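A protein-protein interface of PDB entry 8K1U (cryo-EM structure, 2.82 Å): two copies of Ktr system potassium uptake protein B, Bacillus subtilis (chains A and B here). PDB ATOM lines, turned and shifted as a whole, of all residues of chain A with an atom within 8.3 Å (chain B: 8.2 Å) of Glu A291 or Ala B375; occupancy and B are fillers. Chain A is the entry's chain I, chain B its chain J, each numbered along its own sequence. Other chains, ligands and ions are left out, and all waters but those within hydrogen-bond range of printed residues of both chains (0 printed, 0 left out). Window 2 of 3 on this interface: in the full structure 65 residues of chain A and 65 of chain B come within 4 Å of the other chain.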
ATOM      1  N   LEU A 249     -13.050  14.037 -12.385  1.00  0.00           N
ATOM      2  CA  LEU A 249     -14.257  14.842 -12.211  1.00  0.00           C
ATOM      3  C   LEU A 249     -14.311  16.005 -13.197  1.00  0.00           C
ATOM      4  O   LEU A 249     -15.393  16.370 -13.671  1.00  0.00           O
ATOM      5  CB  LEU A 249     -14.342  15.357 -10.773  1.00  0.00           C
ATOM      6  CG  LEU A 249     -15.126  14.529  -9.750  1.00  0.00           C
ATOM      7  CD1 LEU A 249     -14.553  13.130  -9.582  1.00  0.00           C
ATOM      8  CD2 LEU A 249     -15.164  15.248  -8.412  1.00  0.00           C
ATOM      9  N   GLU A 250     -13.163  16.598 -13.515  1.00  0.00           N
ATOM     10  CA  GLU A 250     -13.110  17.793 -14.347  1.00  0.00           C
ATOM     11  C   GLU A 250     -12.760  17.496 -15.799  1.00  0.00           C
ATOM     12  O   GLU A 250     -12.505  18.432 -16.563  1.00  0.00           O
ATOM     13  CB  GLU A 250     -12.108  18.792 -13.764  1.00  0.00           C
ATOM     14  CG  GLU A 250     -12.455  19.277 -12.367  1.00  0.00           C
ATOM     15  CD  GLU A 250     -13.663  20.192 -12.351  1.00  0.00           C
ATOM     16  OE1 GLU A 250     -13.896  20.888 -13.360  1.00  0.00           O
ATOM     17  OE2 GLU A 250     -14.380  20.215 -11.328  1.00  0.00           O
ATOM     18  N   ASN A 253     -15.642  18.799 -17.910  1.00  0.00           N
ATOM     19  CA  ASN A 253     -16.103  20.134 -17.546  1.00  0.00           C
ATOM     20  C   ASN A 253     -15.691  21.136 -18.616  1.00  0.00           C
ATOM     21  O   ASN A 253     -14.502  21.223 -18.941  1.00  0.00           O
ATOM     22  CB  ASN A 253     -15.533  20.541 -16.192  1.00  0.00           C
ATOM     23  CG  ASN A 253     -16.016  21.906 -15.744  1.00  0.00           C
ATOM     24  OD1 ASN A 253     -15.370  22.921 -16.005  1.00  0.00           O
ATOM     25  ND2 ASN A 253     -17.157  21.938 -15.065  1.00  0.00           N
ATOM     26  N   PHE A 286     -11.464  28.189 -10.037  1.00  0.00           N
ATOM     27  CA  PHE A 286     -12.203  27.400  -9.059  1.00  0.00           C
ATOM     28  C   PHE A 286     -13.684  27.752  -9.027  1.00  0.00           C
ATOM     29  O   PHE A 286     -14.488  26.951  -8.539  1.00  0.00           O
ATOM     30  CB  PHE A 286     -11.594  27.577  -7.667  1.00  0.00           C
ATOM     31  CG  PHE A 286     -10.433  26.664  -7.392  1.00  0.00           C
ATOM     32  CD1 PHE A 286      -9.178  26.939  -7.910  1.00  0.00           C
ATOM     33  CD2 PHE A 286     -10.598  25.529  -6.613  1.00  0.00           C
ATOM     34  CE1 PHE A 286      -8.107  26.098  -7.658  1.00  0.00           C
ATOM     35  CE2 PHE A 286      -9.533  24.685  -6.357  1.00  0.00           C
ATOM     36  CZ  PHE A 286      -8.286  24.971  -6.879  1.00  0.00           C
ATOM     37  N   GLY A 287     -14.065  28.927  -9.534  1.00  0.00           N
ATOM     38  CA  GLY A 287     -15.470  29.291  -9.580  1.00  0.00           C
ATOM     39  C   GLY A 287     -16.265  28.546 -10.631  1.00  0.00           C
ATOM     40  O   GLY A 287     -17.491  28.457 -10.517  1.00  0.00           O
ATOM     41  N   SER A 288     -15.596  28.009 -11.649  1.00  0.00           N
ATOM     42  CA  SER A 288     -16.253  27.271 -12.718  1.00  0.00           C
ATOM     43  C   SER A 288     -16.113  25.761 -12.575  1.00  0.00           C
ATOM     44  O   SER A 288     -16.550  25.026 -13.465  1.00  0.00           O
ATOM     45  CB  SER A 288     -15.707  27.717 -14.078  1.00  0.00           C
ATOM     46  OG  SER A 288     -14.294  27.633 -14.112  1.00  0.00           O
ATOM     47  N   MET A 289     -15.516  25.283 -11.488  1.00  0.00           N
ATOM     48  CA  MET A 289     -15.408  23.852 -11.262  1.00  0.00           C
ATOM     49  C   MET A 289     -16.742  23.282 -10.788  1.00  0.00           C
ATOM     50  O   MET A 289     -17.621  24.000 -10.305  1.00  0.00           O
ATOM     51  CB  MET A 289     -14.315  23.543 -10.237  1.00  0.00           C
ATOM     52  CG  MET A 289     -12.898  23.707 -10.756  1.00  0.00           C
ATOM     53  SD  MET A 289     -11.663  23.196  -9.546  1.00  0.00           S
ATOM     54  CE  MET A 289     -10.156  23.368 -10.497  1.00  0.00           C
ATOM     55  N   ARG A 290     -16.885  21.967 -10.938  1.00  0.00           N
ATOM     56  CA  ARG A 290     -18.080  21.289 -10.468  1.00  0.00           C
ATOM     57  C   ARG A 290     -18.099  21.234  -8.943  1.00  0.00           C
ATOM     58  O   ARG A 290     -17.073  21.392  -8.274  1.00  0.00           O
ATOM     59  CB  ARG A 290     -18.162  19.875 -11.044  1.00  0.00           C
ATOM     60  CG  ARG A 290     -18.389  19.822 -12.543  1.00  0.00           C
ATOM     61  CD  ARG A 290     -18.725  18.407 -12.988  1.00  0.00           C
ATOM     62  NE  ARG A 290     -19.050  18.337 -14.407  1.00  0.00           N
ATOM     63  CZ  ARG A 290     -18.194  17.983 -15.355  1.00  0.00           C
ATOM     64  NH1 ARG A 290     -16.944  17.655 -15.071  1.00  0.00           N
ATOM     65  NH2 ARG A 290     -18.603  17.953 -16.620  1.00  0.00           N
ATOM     66  N   GLU A 291     -19.296  21.009  -8.393  1.00  0.00           N
ATOM     67  CA  GLU A 291     -19.451  20.972  -6.942  1.00  0.00           C
ATOM     68  C   GLU A 291     -18.749  19.770  -6.322  1.00  0.00           C
ATOM     69  O   GLU A 291     -18.351  19.828  -5.154  1.00  0.00           O
ATOM     70  CB  GLU A 291     -20.933  20.965  -6.569  1.00  0.00           C
ATOM     71  CG  GLU A 291     -21.672  22.241  -6.932  1.00  0.00           C
ATOM     72  CD  GLU A 291     -23.117  22.229  -6.471  1.00  0.00           C
ATOM     73  OE1 GLU A 291     -23.588  21.168  -6.012  1.00  0.00           O
ATOM     74  OE2 GLU A 291     -23.780  23.283  -6.566  1.00  0.00           O
ATOM     75  N   GLY A 292     -18.595  18.680  -7.076  1.00  0.00           N
ATOM     76  CA  GLY A 292     -17.939  17.501  -6.532  1.00  0.00           C
ATOM     77  C   GLY A 292     -16.468  17.724  -6.237  1.00  0.00           C
ATOM     78  O   GLY A 292     -15.950  17.247  -5.223  1.00  0.00           O
ATOM     79  N   THR A 293     -15.773  18.449  -7.117  1.00  0.00           N
ATOM     80  CA  THR A 293     -14.359  18.730  -6.895  1.00  0.00           C
ATOM     81  C   THR A 293     -14.159  19.734  -5.765  1.00  0.00           C
ATOM     82  O   THR A 293     -13.159  19.663  -5.041  1.00  0.00           O
ATOM     83  CB  THR A 293     -13.717  19.243  -8.186  1.00  0.00           C
ATOM     84  OG1 THR A 293     -14.145  18.429  -9.285  1.00  0.00           O
ATOM     85  CG2 THR A 293     -12.199  19.184  -8.094  1.00  0.00           C
ATOM     86  N   ILE A 294     -15.099  20.667  -5.596  1.00  0.00           N
ATOM     87  CA  ILE A 294     -14.994  21.654  -4.526  1.00  0.00           C
ATOM     88  C   ILE A 294     -15.162  20.990  -3.164  1.00  0.00           C
ATOM     89  O   ILE A 294     -14.480  21.349  -2.196  1.00  0.00           O
ATOM     90  CB  ILE A 294     -16.019  22.781  -4.752  1.00  0.00           C
ATOM     91  CG1 ILE A 294     -15.763  23.458  -6.099  1.00  0.00           C
ATOM     92  CG2 ILE A 294     -15.960  23.805  -3.633  1.00  0.00           C
ATOM     93  CD1 ILE A 294     -16.780  24.512  -6.458  1.00  0.00           C
ATOM     94  N   VAL A 295     -16.062  20.006  -3.069  1.00  0.00           N
ATOM     95  CA  VAL A 295     -16.258  19.282  -1.813  1.00  0.00           C
ATOM     96  C   VAL A 295     -14.999  18.508  -1.438  1.00  0.00           C
ATOM     97  O   VAL A 295     -14.572  18.514  -0.277  1.00  0.00           O
ATOM     98  CB  VAL A 295     -17.487  18.358  -1.916  1.00  0.00           C
ATOM     99  CG1 VAL A 295     -17.559  17.418  -0.725  1.00  0.00           C
ATOM    100  CG2 VAL A 295     -18.756  19.180  -2.006  1.00  0.00           C
ATOM    101  N   PHE A 296     -14.378  17.841  -2.415  1.00  0.00           N
ATOM    102  CA  PHE A 296     -13.131  17.133  -2.148  1.00  0.00           C
ATOM    103  C   PHE A 296     -12.001  18.098  -1.809  1.00  0.00           C
ATOM    104  O   PHE A 296     -11.115  17.757  -1.017  1.00  0.00           O
ATOM    105  CB  PHE A 296     -12.745  16.265  -3.346  1.00  0.00           C
ATOM    106  CG  PHE A 296     -11.510  15.439  -3.122  1.00  0.00           C
ATOM    107  CD1 PHE A 296     -11.565  14.277  -2.368  1.00  0.00           C
ATOM    108  CD2 PHE A 296     -10.292  15.823  -3.666  1.00  0.00           C
ATOM    109  CE1 PHE A 296     -10.432  13.515  -2.157  1.00  0.00           C
ATOM    110  CE2 PHE A 296      -9.156  15.065  -3.458  1.00  0.00           C
ATOM    111  CZ  PHE A 296      -9.226  13.910  -2.703  1.00  0.00           C
ATOM    112  N   THR A 297     -12.014  19.295  -2.397  1.00  0.00           N
ATOM    113  CA  THR A 297     -11.021  20.306  -2.051  1.00  0.00           C
ATOM    114  C   THR A 297     -11.218  20.816  -0.628  1.00  0.00           C
ATOM    115  O   THR A 297     -10.240  21.176   0.038  1.00  0.00           O
ATOM    116  CB  THR A 297     -11.084  21.463  -3.051  1.00  0.00           C
ATOM    117  OG1 THR A 297     -11.169  20.939  -4.382  1.00  0.00           O
ATOM    118  CG2 THR A 297      -9.843  22.339  -2.947  1.00  0.00           C
ATOM    119  N   LEU A 298     -12.466  20.844  -0.148  1.00  0.00           N
ATOM    120  CA  LEU A 298     -12.742  21.282   1.219  1.00  0.00           C
ATOM    121  C   LEU A 298     -12.062  20.379   2.240  1.00  0.00           C
ATOM    122  O   LEU A 298     -11.457  20.863   3.202  1.00  0.00           O
ATOM    123  CB  LEU A 298     -14.250  21.311   1.461  1.00  0.00           C
ATOM    124  CG  LEU A 298     -14.975  22.657   1.457  1.00  0.00           C
ATOM    125  CD1 LEU A 298     -14.547  23.508   0.281  1.00  0.00           C
ATOM    126  CD2 LEU A 298     -16.474  22.424   1.420  1.00  0.00           C
ATOM    127  N   LEU A 378     -21.941  27.761  -1.045  1.00  0.00           N
ATOM    128  CA  LEU A 378     -20.716  27.039  -1.378  1.00  0.00           C
ATOM    129  C   LEU A 378     -19.501  27.958  -1.343  1.00  0.00           C
ATOM    130  O   LEU A 378     -18.412  27.540  -0.931  1.00  0.00           O
ATOM    131  CB  LEU A 378     -20.855  26.377  -2.749  1.00  0.00           C
ATOM    132  CG  LEU A 378     -19.684  25.507  -3.212  1.00  0.00           C
ATOM    133  CD1 LEU A 378     -19.360  24.444  -2.175  1.00  0.00           C
ATOM    134  CD2 LEU A 378     -19.996  24.868  -4.553  1.00  0.00           C
ATOM    135  N   MET A 395     -13.454  31.416  -4.741  1.00  0.00           N
ATOM    136  CA  MET A 395     -14.494  31.158  -5.726  1.00  0.00           C
ATOM    137  C   MET A 395     -15.136  32.440  -6.240  1.00  0.00           C
ATOM    138  O   MET A 395     -16.053  32.373  -7.065  1.00  0.00           O
ATOM    139  CB  MET A 395     -15.568  30.236  -5.142  1.00  0.00           C
ATOM    140  CG  MET A 395     -15.132  28.787  -4.992  1.00  0.00           C
ATOM    141  SD  MET A 395     -16.458  27.717  -4.402  1.00  0.00           S
ATOM    142  CE  MET A 395     -17.723  28.042  -5.626  1.00  0.00           C
ATOM    143  N   ILE B 366     -22.525  13.808   1.008  1.00  0.00           N
ATOM    144  CA  ILE B 366     -22.510  15.090   0.309  1.00  0.00           C
ATOM    145  C   ILE B 366     -21.694  14.988  -0.974  1.00  0.00           C
ATOM    146  O   ILE B 366     -22.083  15.526  -2.017  1.00  0.00           O
ATOM    147  CB  ILE B 366     -21.977  16.196   1.238  1.00  0.00           C
ATOM    148  CG1 ILE B 366     -22.862  16.323   2.478  1.00  0.00           C
ATOM    149  CG2 ILE B 366     -21.904  17.530   0.510  1.00  0.00           C
ATOM    150  CD1 ILE B 366     -22.357  17.327   3.488  1.00  0.00           C
ATOM    151  N   PHE B 367     -20.558  14.287  -0.920  1.00  0.00           N
ATOM    152  CA  PHE B 367     -19.721  14.122  -2.104  1.00  0.00           C
ATOM    153  C   PHE B 367     -20.432  13.313  -3.183  1.00  0.00           C
ATOM    154  O   PHE B 367     -20.318  13.624  -4.374  1.00  0.00           O
ATOM    155  CB  PHE B 367     -18.398  13.458  -1.719  1.00  0.00           C
ATOM    156  CG  PHE B 367     -17.451  13.269  -2.873  1.00  0.00           C
ATOM    157  CD1 PHE B 367     -16.710  14.334  -3.358  1.00  0.00           C
ATOM    158  CD2 PHE B 367     -17.296  12.026  -3.465  1.00  0.00           C
ATOM    159  CE1 PHE B 367     -15.838  14.165  -4.417  1.00  0.00           C
ATOM    160  CE2 PHE B 367     -16.425  11.849  -4.524  1.00  0.00           C
ATOM    161  CZ  PHE B 367     -15.695  12.921  -5.000  1.00  0.00           C
ATOM    162  N   LEU B 369     -23.776  12.986  -3.543  1.00  0.00           N
ATOM    163  CA  LEU B 369     -24.960  13.681  -4.039  1.00  0.00           C
ATOM    164  C   LEU B 369     -24.598  14.833  -4.967  1.00  0.00           C
ATOM    165  O   LEU B 369     -25.367  15.150  -5.882  1.00  0.00           O
ATOM    166  CB  LEU B 369     -25.804  14.191  -2.872  1.00  0.00           C
ATOM    167  CG  LEU B 369     -26.657  13.165  -2.127  1.00  0.00           C
ATOM    168  CD1 LEU B 369     -27.415  13.833  -0.994  1.00  0.00           C
ATOM    169  CD2 LEU B 369     -27.616  12.465  -3.078  1.00  0.00           C
ATOM    170  N   THR B 370     -23.448  15.476  -4.747  1.00  0.00           N
ATOM    171  CA  THR B 370     -23.028  16.556  -5.634  1.00  0.00           C
ATOM    172  C   THR B 370     -22.668  16.033  -7.018  1.00  0.00           C
ATOM    173  O   THR B 370     -22.883  16.725  -8.021  1.00  0.00           O
ATOM    174  CB  THR B 370     -21.845  17.311  -5.026  1.00  0.00           C
ATOM    175  OG1 THR B 370     -20.882  16.375  -4.527  1.00  0.00           O
ATOM    176  CG2 THR B 370     -22.310  18.217  -3.894  1.00  0.00           C
ATOM    177  N   ILE B 371     -22.114  14.821  -7.092  1.00  0.00           N
ATOM    178  CA  ILE B 371     -21.831  14.202  -8.383  1.00  0.00           C
ATOM    179  C   ILE B 371     -23.127  13.875  -9.116  1.00  0.00           C
ATOM    180  O   ILE B 371     -23.253  14.119 -10.322  1.00  0.00           O
ATOM    181  CB  ILE B 371     -20.958  12.948  -8.188  1.00  0.00           C
ATOM    182  CG1 ILE B 371     -19.610  13.326  -7.571  1.00  0.00           C
ATOM    183  CG2 ILE B 371     -20.756  12.216  -9.506  1.00  0.00           C
ATOM    184  CD1 ILE B 371     -18.800  14.284  -8.415  1.00  0.00           C
ATOM    185  N   THR B 372     -24.113  13.335  -8.401  1.00  0.00           N
ATOM    186  CA  THR B 372     -25.351  12.864  -9.016  1.00  0.00           C
ATOM    187  C   THR B 372     -26.372  13.986  -9.193  1.00  0.00           C
ATOM    188  O   THR B 372     -26.805  14.269 -10.314  1.00  0.00           O
ATOM    189  CB  THR B 372     -25.951  11.731  -8.177  1.00  0.00           C
ATOM    190  OG1 THR B 372     -25.012  10.653  -8.083  1.00  0.00           O
ATOM    191  CG2 THR B 372     -27.238  11.225  -8.809  1.00  0.00           C
ATOM    192  N   GLU B 373     -26.762  14.631  -8.097  1.00  0.00           N
ATOM    193  CA  GLU B 373     -27.859  15.585  -8.131  1.00  0.00           C
ATOM    194  C   GLU B 373     -27.395  16.956  -8.608  1.00  0.00           C
ATOM    195  O   GLU B 373     -26.299  17.420  -8.278  1.00  0.00           O
ATOM    196  CB  GLU B 373     -28.501  15.711  -6.748  1.00  0.00           C
ATOM    197  CG  GLU B 373     -29.180  14.441  -6.265  1.00  0.00           C
ATOM    198  CD  GLU B 373     -30.383  14.067  -7.109  1.00  0.00           C
ATOM    199  OE1 GLU B 373     -31.077  14.981  -7.602  1.00  0.00           O
ATOM    200  OE2 GLU B 373     -30.632  12.856  -7.285  1.00  0.00           O
ATOM    201  N   GLN B 374     -28.250  17.603  -9.396  1.00  0.00           N
ATOM    202  CA  GLN B 374     -28.057  18.983  -9.835  1.00  0.00           C
ATOM    203  C   GLN B 374     -28.966  19.851  -8.972  1.00  0.00           C
ATOM    204  O   GLN B 374     -30.157  19.996  -9.258  1.00  0.00           O
ATOM    205  CB  GLN B 374     -28.372  19.137 -11.320  1.00  0.00           C
ATOM    206  CG  GLN B 374     -27.638  18.156 -12.221  1.00  0.00           C
ATOM    207  CD  GLN B 374     -26.139  18.389 -12.247  1.00  0.00           C
ATOM    208  OE1 GLN B 374     -25.668  19.511 -12.059  1.00  0.00           O
ATOM    209  NE2 GLN B 374     -25.380  17.325 -12.483  1.00  0.00           N
ATOM    210  N   ALA B 375     -28.401  20.424  -7.916  1.00  0.00           N
ATOM    211  CA  ALA B 375     -29.176  21.127  -6.905  1.00  0.00           C
ATOM    212  C   ALA B 375     -28.276  22.154  -6.239  1.00  0.00           C
ATOM    213  O   ALA B 375     -27.046  22.065  -6.344  1.00  0.00           O
ATOM    214  CB  ALA B 375     -29.743  20.148  -5.867  1.00  0.00           C
ATOM    215  N   PRO B 376     -28.853  23.159  -5.572  1.00  0.00           N
ATOM    216  CA  PRO B 376     -28.033  24.069  -4.766  1.00  0.00           C
ATOM    217  C   PRO B 376     -27.298  23.326  -3.660  1.00  0.00           C
ATOM    218  O   PRO B 376     -27.776  22.322  -3.128  1.00  0.00           O
ATOM    219  CB  PRO B 376     -29.055  25.056  -4.195  1.00  0.00           C
ATOM    220  CG  PRO B 376     -30.148  25.068  -5.200  1.00  0.00           C
ATOM    221  CD  PRO B 376     -30.232  23.661  -5.726  1.00  0.00           C
ATOM    222  N   PHE B 377     -26.106  23.831  -3.329  1.00  0.00           N
ATOM    223  CA  PHE B 377     -25.233  23.142  -2.386  1.00  0.00           C
ATOM    224  C   PHE B 377     -25.809  23.125  -0.975  1.00  0.00           C
ATOM    225  O   PHE B 377     -25.589  22.160  -0.235  1.00  0.00           O
ATOM    226  CB  PHE B 377     -23.849  23.793  -2.389  1.00  0.00           C
ATOM    227  CG  PHE B 377     -22.865  23.133  -1.467  1.00  0.00           C
ATOM    228  CD1 PHE B 377     -22.364  21.875  -1.756  1.00  0.00           C
ATOM    229  CD2 PHE B 377     -22.434  23.776  -0.318  1.00  0.00           C
ATOM    230  CE1 PHE B 377     -21.456  21.267  -0.911  1.00  0.00           C
ATOM    231  CE2 PHE B 377     -21.526  23.174   0.531  1.00  0.00           C
ATOM    232  CZ  PHE B 377     -21.034  21.918   0.233  1.00  0.00           C
ATOM    233  N   LEU B 378     -26.537  24.174  -0.584  1.00  0.00           N
ATOM    234  CA  LEU B 378     -27.111  24.216   0.758  1.00  0.00           C
ATOM    235  C   LEU B 378     -28.188  23.151   0.936  1.00  0.00           C
ATOM    236  O   LEU B 378     -28.314  22.563   2.017  1.00  0.00           O
ATOM    237  CB  LEU B 378     -27.674  25.607   1.043  1.00  0.00           C
ATOM    238  CG  LEU B 378     -28.241  25.844   2.446  1.00  0.00           C
ATOM    239  CD1 LEU B 378     -27.211  25.496   3.507  1.00  0.00           C
ATOM    240  CD2 LEU B 378     -28.697  27.285   2.596  1.00  0.00           C
ATOM    241  N   GLN B 379     -28.973  22.888  -0.114  1.00  0.00           N
ATOM    242  CA  GLN B 379     -30.000  21.854  -0.032  1.00  0.00           C
ATOM    243  C   GLN B 379     -29.393  20.457   0.022  1.00  0.00           C
ATOM    244  O   GLN B 379     -29.966  19.560   0.652  1.00  0.00           O
ATOM    245  CB  GLN B 379     -30.957  21.967  -1.219  1.00  0.00           C
ATOM    246  CG  GLN B 379     -31.720  23.281  -1.288  1.00  0.00           C
ATOM    247  CD  GLN B 379     -32.686  23.331  -2.456  1.00  0.00           C
ATOM    248  OE1 GLN B 379     -32.816  22.369  -3.212  1.00  0.00           O
ATOM    249  NE2 GLN B 379     -33.370  24.459  -2.610  1.00  0.00           N
ATOM    250  N   ILE B 380     -28.251  20.250  -0.637  1.00  0.00           N
ATOM    251  CA  ILE B 380     -27.602  18.942  -0.618  1.00  0.00           C
ATOM    252  C   ILE B 380     -27.063  18.631   0.773  1.00  0.00           C
ATOM    253  O   ILE B 380     -27.235  17.517   1.285  1.00  0.00           O
ATOM    254  CB  ILE B 380     -26.494  18.889  -1.686  1.00  0.00           C
ATOM    255  CG1 ILE B 380     -27.105  18.970  -3.087  1.00  0.00           C
ATOM    256  CG2 ILE B 380     -25.651  17.632  -1.533  1.00  0.00           C
ATOM    257  CD1 ILE B 380     -26.091  18.884  -4.204  1.00  0.00           C
ATOM    258  N   VAL B 381     -26.413  19.608   1.409  1.00  0.00           N
ATOM    259  CA  VAL B 381     -25.869  19.402   2.748  1.00  0.00           C
ATOM    260  C   VAL B 381     -26.993  19.247   3.767  1.00  0.00           C
ATOM    261  O   VAL B 381     -26.899  18.433   4.694  1.00  0.00           O
ATOM    262  CB  VAL B 381     -24.917  20.557   3.115  1.00  0.00           C
ATOM    263  CG1 VAL B 381     -24.317  20.347   4.491  1.00  0.00           C
ATOM    264  CG2 VAL B 381     -23.819  20.676   2.079  1.00  0.00           C
ATOM    265  N   GLY B 396     -36.541  21.193  -0.120  1.00  0.00           N
ATOM    266  CA  GLY B 396     -37.106  21.108  -1.451  1.00  0.00           C
ATOM    267  C   GLY B 396     -36.303  20.233  -2.391  1.00  0.00           C
ATOM    268  O   GLY B 396     -36.271  20.480  -3.600  1.00  0.00           O
ATOM    269  N   LEU B 397     -35.647  19.207  -1.850  1.00  0.00           N
ATOM    270  CA  LEU B 397     -34.780  18.336  -2.635  1.00  0.00           C
ATOM    271  C   LEU B 397     -35.293  16.909  -2.767  1.00  0.00           C
ATOM    272  O   LEU B 397     -35.070  16.286  -3.807  1.00  0.00           O
ATOM    273  CB  LEU B 397     -33.372  18.306  -2.024  1.00  0.00           C
ATOM    274  CG  LEU B 397     -32.283  17.507  -2.746  1.00  0.00           C
ATOM    275  CD1 LEU B 397     -32.185  17.927  -4.204  1.00  0.00           C
ATOM    276  CD2 LEU B 397     -30.942  17.671  -2.051  1.00  0.00           C
ATOM    277  N   GLU B 400     -37.291  16.052  -5.753  1.00  0.00           N
ATOM    278  CA  GLU B 400     -36.502  16.291  -6.953  1.00  0.00           C
ATOM    279  C   GLU B 400     -35.324  15.336  -7.095  1.00  0.00           C
ATOM    280  O   GLU B 400     -34.530  15.492  -8.028  1.00  0.00           O
ATOM    281  CB  GLU B 400     -35.995  17.737  -6.969  1.00  0.00           C
ATOM    282  CG  GLU B 400     -37.079  18.782  -6.743  1.00  0.00           C
ATOM    283  CD  GLU B 400     -38.098  18.829  -7.867  1.00  0.00           C
ATOM    284  OE1 GLU B 400     -37.732  18.526  -9.022  1.00  0.00           O
ATOM    285  OE2 GLU B 400     -39.267  19.173  -7.593  1.00  0.00           O
ATOM    286  N   LEU B 401     -35.186  14.364  -6.197  1.00  0.00           N
ATOM    287  CA  LEU B 401     -34.076  13.423  -6.273  1.00  0.00           C
ATOM    288  C   LEU B 401     -34.237  12.486  -7.463  1.00  0.00           C
ATOM    289  O   LEU B 401     -35.351  12.093  -7.823  1.00  0.00           O
ATOM    290  CB  LEU B 401     -33.977  12.612  -4.981  1.00  0.00           C
ATOM    291  CG  LEU B 401     -33.514  13.357  -3.727  1.00  0.00           C
ATOM    292  CD1 LEU B 401     -33.555  12.443  -2.513  1.00  0.00           C
ATOM    293  CD2 LEU B 401     -32.118  13.925  -3.926  1.00  0.00           C
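OE2 of Glu A291 lies close to O of Ala B375 (3.5 Å).
The guanidinium group (NH1) of Arg A290 sits at hydrogen-bond distance from the backbone carbonyl oxygen (O) of Leu A249, 2.5 Å away.
The side-chain hydroxyl (OG1) of Thr B370 is in hydrogen-bond range of the backbone carbonyl oxygen (O) of Ile B366, 2.9 Å away.
The backbone carbonyl oxygen of Phe B367 lies within hydrogen-bond range of the side-chain hydroxyl of Thr B370 (2.8 Å).
Among the printed residues, pairs that only touch across the chains: Gly A292 with Phe B367 (3.2 Å), Val A295 with Phe B377 (3.6 Å), Leu A378 with Phe B377 (3.7 Å), Gly A292 with Thr B370 (3.7 Å), Leu A249 with Ile B371 (3.8 Å), Gly A292 with Ile B371 (3.8 Å), Glu A291 with Ile B380 (3.8 Å), Glu A291 with Thr B370 (3.9 Å) and Phe A296 with Phe B367 (3.9 Å).
Printed residues of chain B within 4 Å of Leu A249: Ile B371.
Arg A290 touches none of the printed residues of chain B.
Glu A291 touches three residues of chain B.
Printed residues of chain B within 4 Å of Gly A292: Phe B367 (3.2 Å), Thr B370 (3.7 Å) and Ile B371 (3.8 Å).
Glu B373 touches none of the printed residues of chain A.
Of chain A, only Glu A291 comes within 4 Å of Ala B375.
No residue of chain A comes within 4 Å of Pro B376.
Of the printed residues of chain A, Phe B377 touches Val A295 (3.6 Å) and Leu A378 (3.7 Å).
The nearest residue of chain B that does not touch Glu A291 is Phe B377 (4.02 Å).
The nearest printed residue of chain A that does not touch Ile B380 is Val A295 (7.1 Å).
Hydrophobic or aromatic side chains of chain B that line the printed part of chain A: Phe B367, Ile B371, Phe B377 and Ile B380.
Along chain B the printed residues that touch a printed residue of chain A span positions 367 to 380.
Among the printed residues, no Asp or Glu carboxylate lies within 4 Å of a Lys or Arg side-chain nitrogen of the other chain.
Position printed for both chains: 378.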
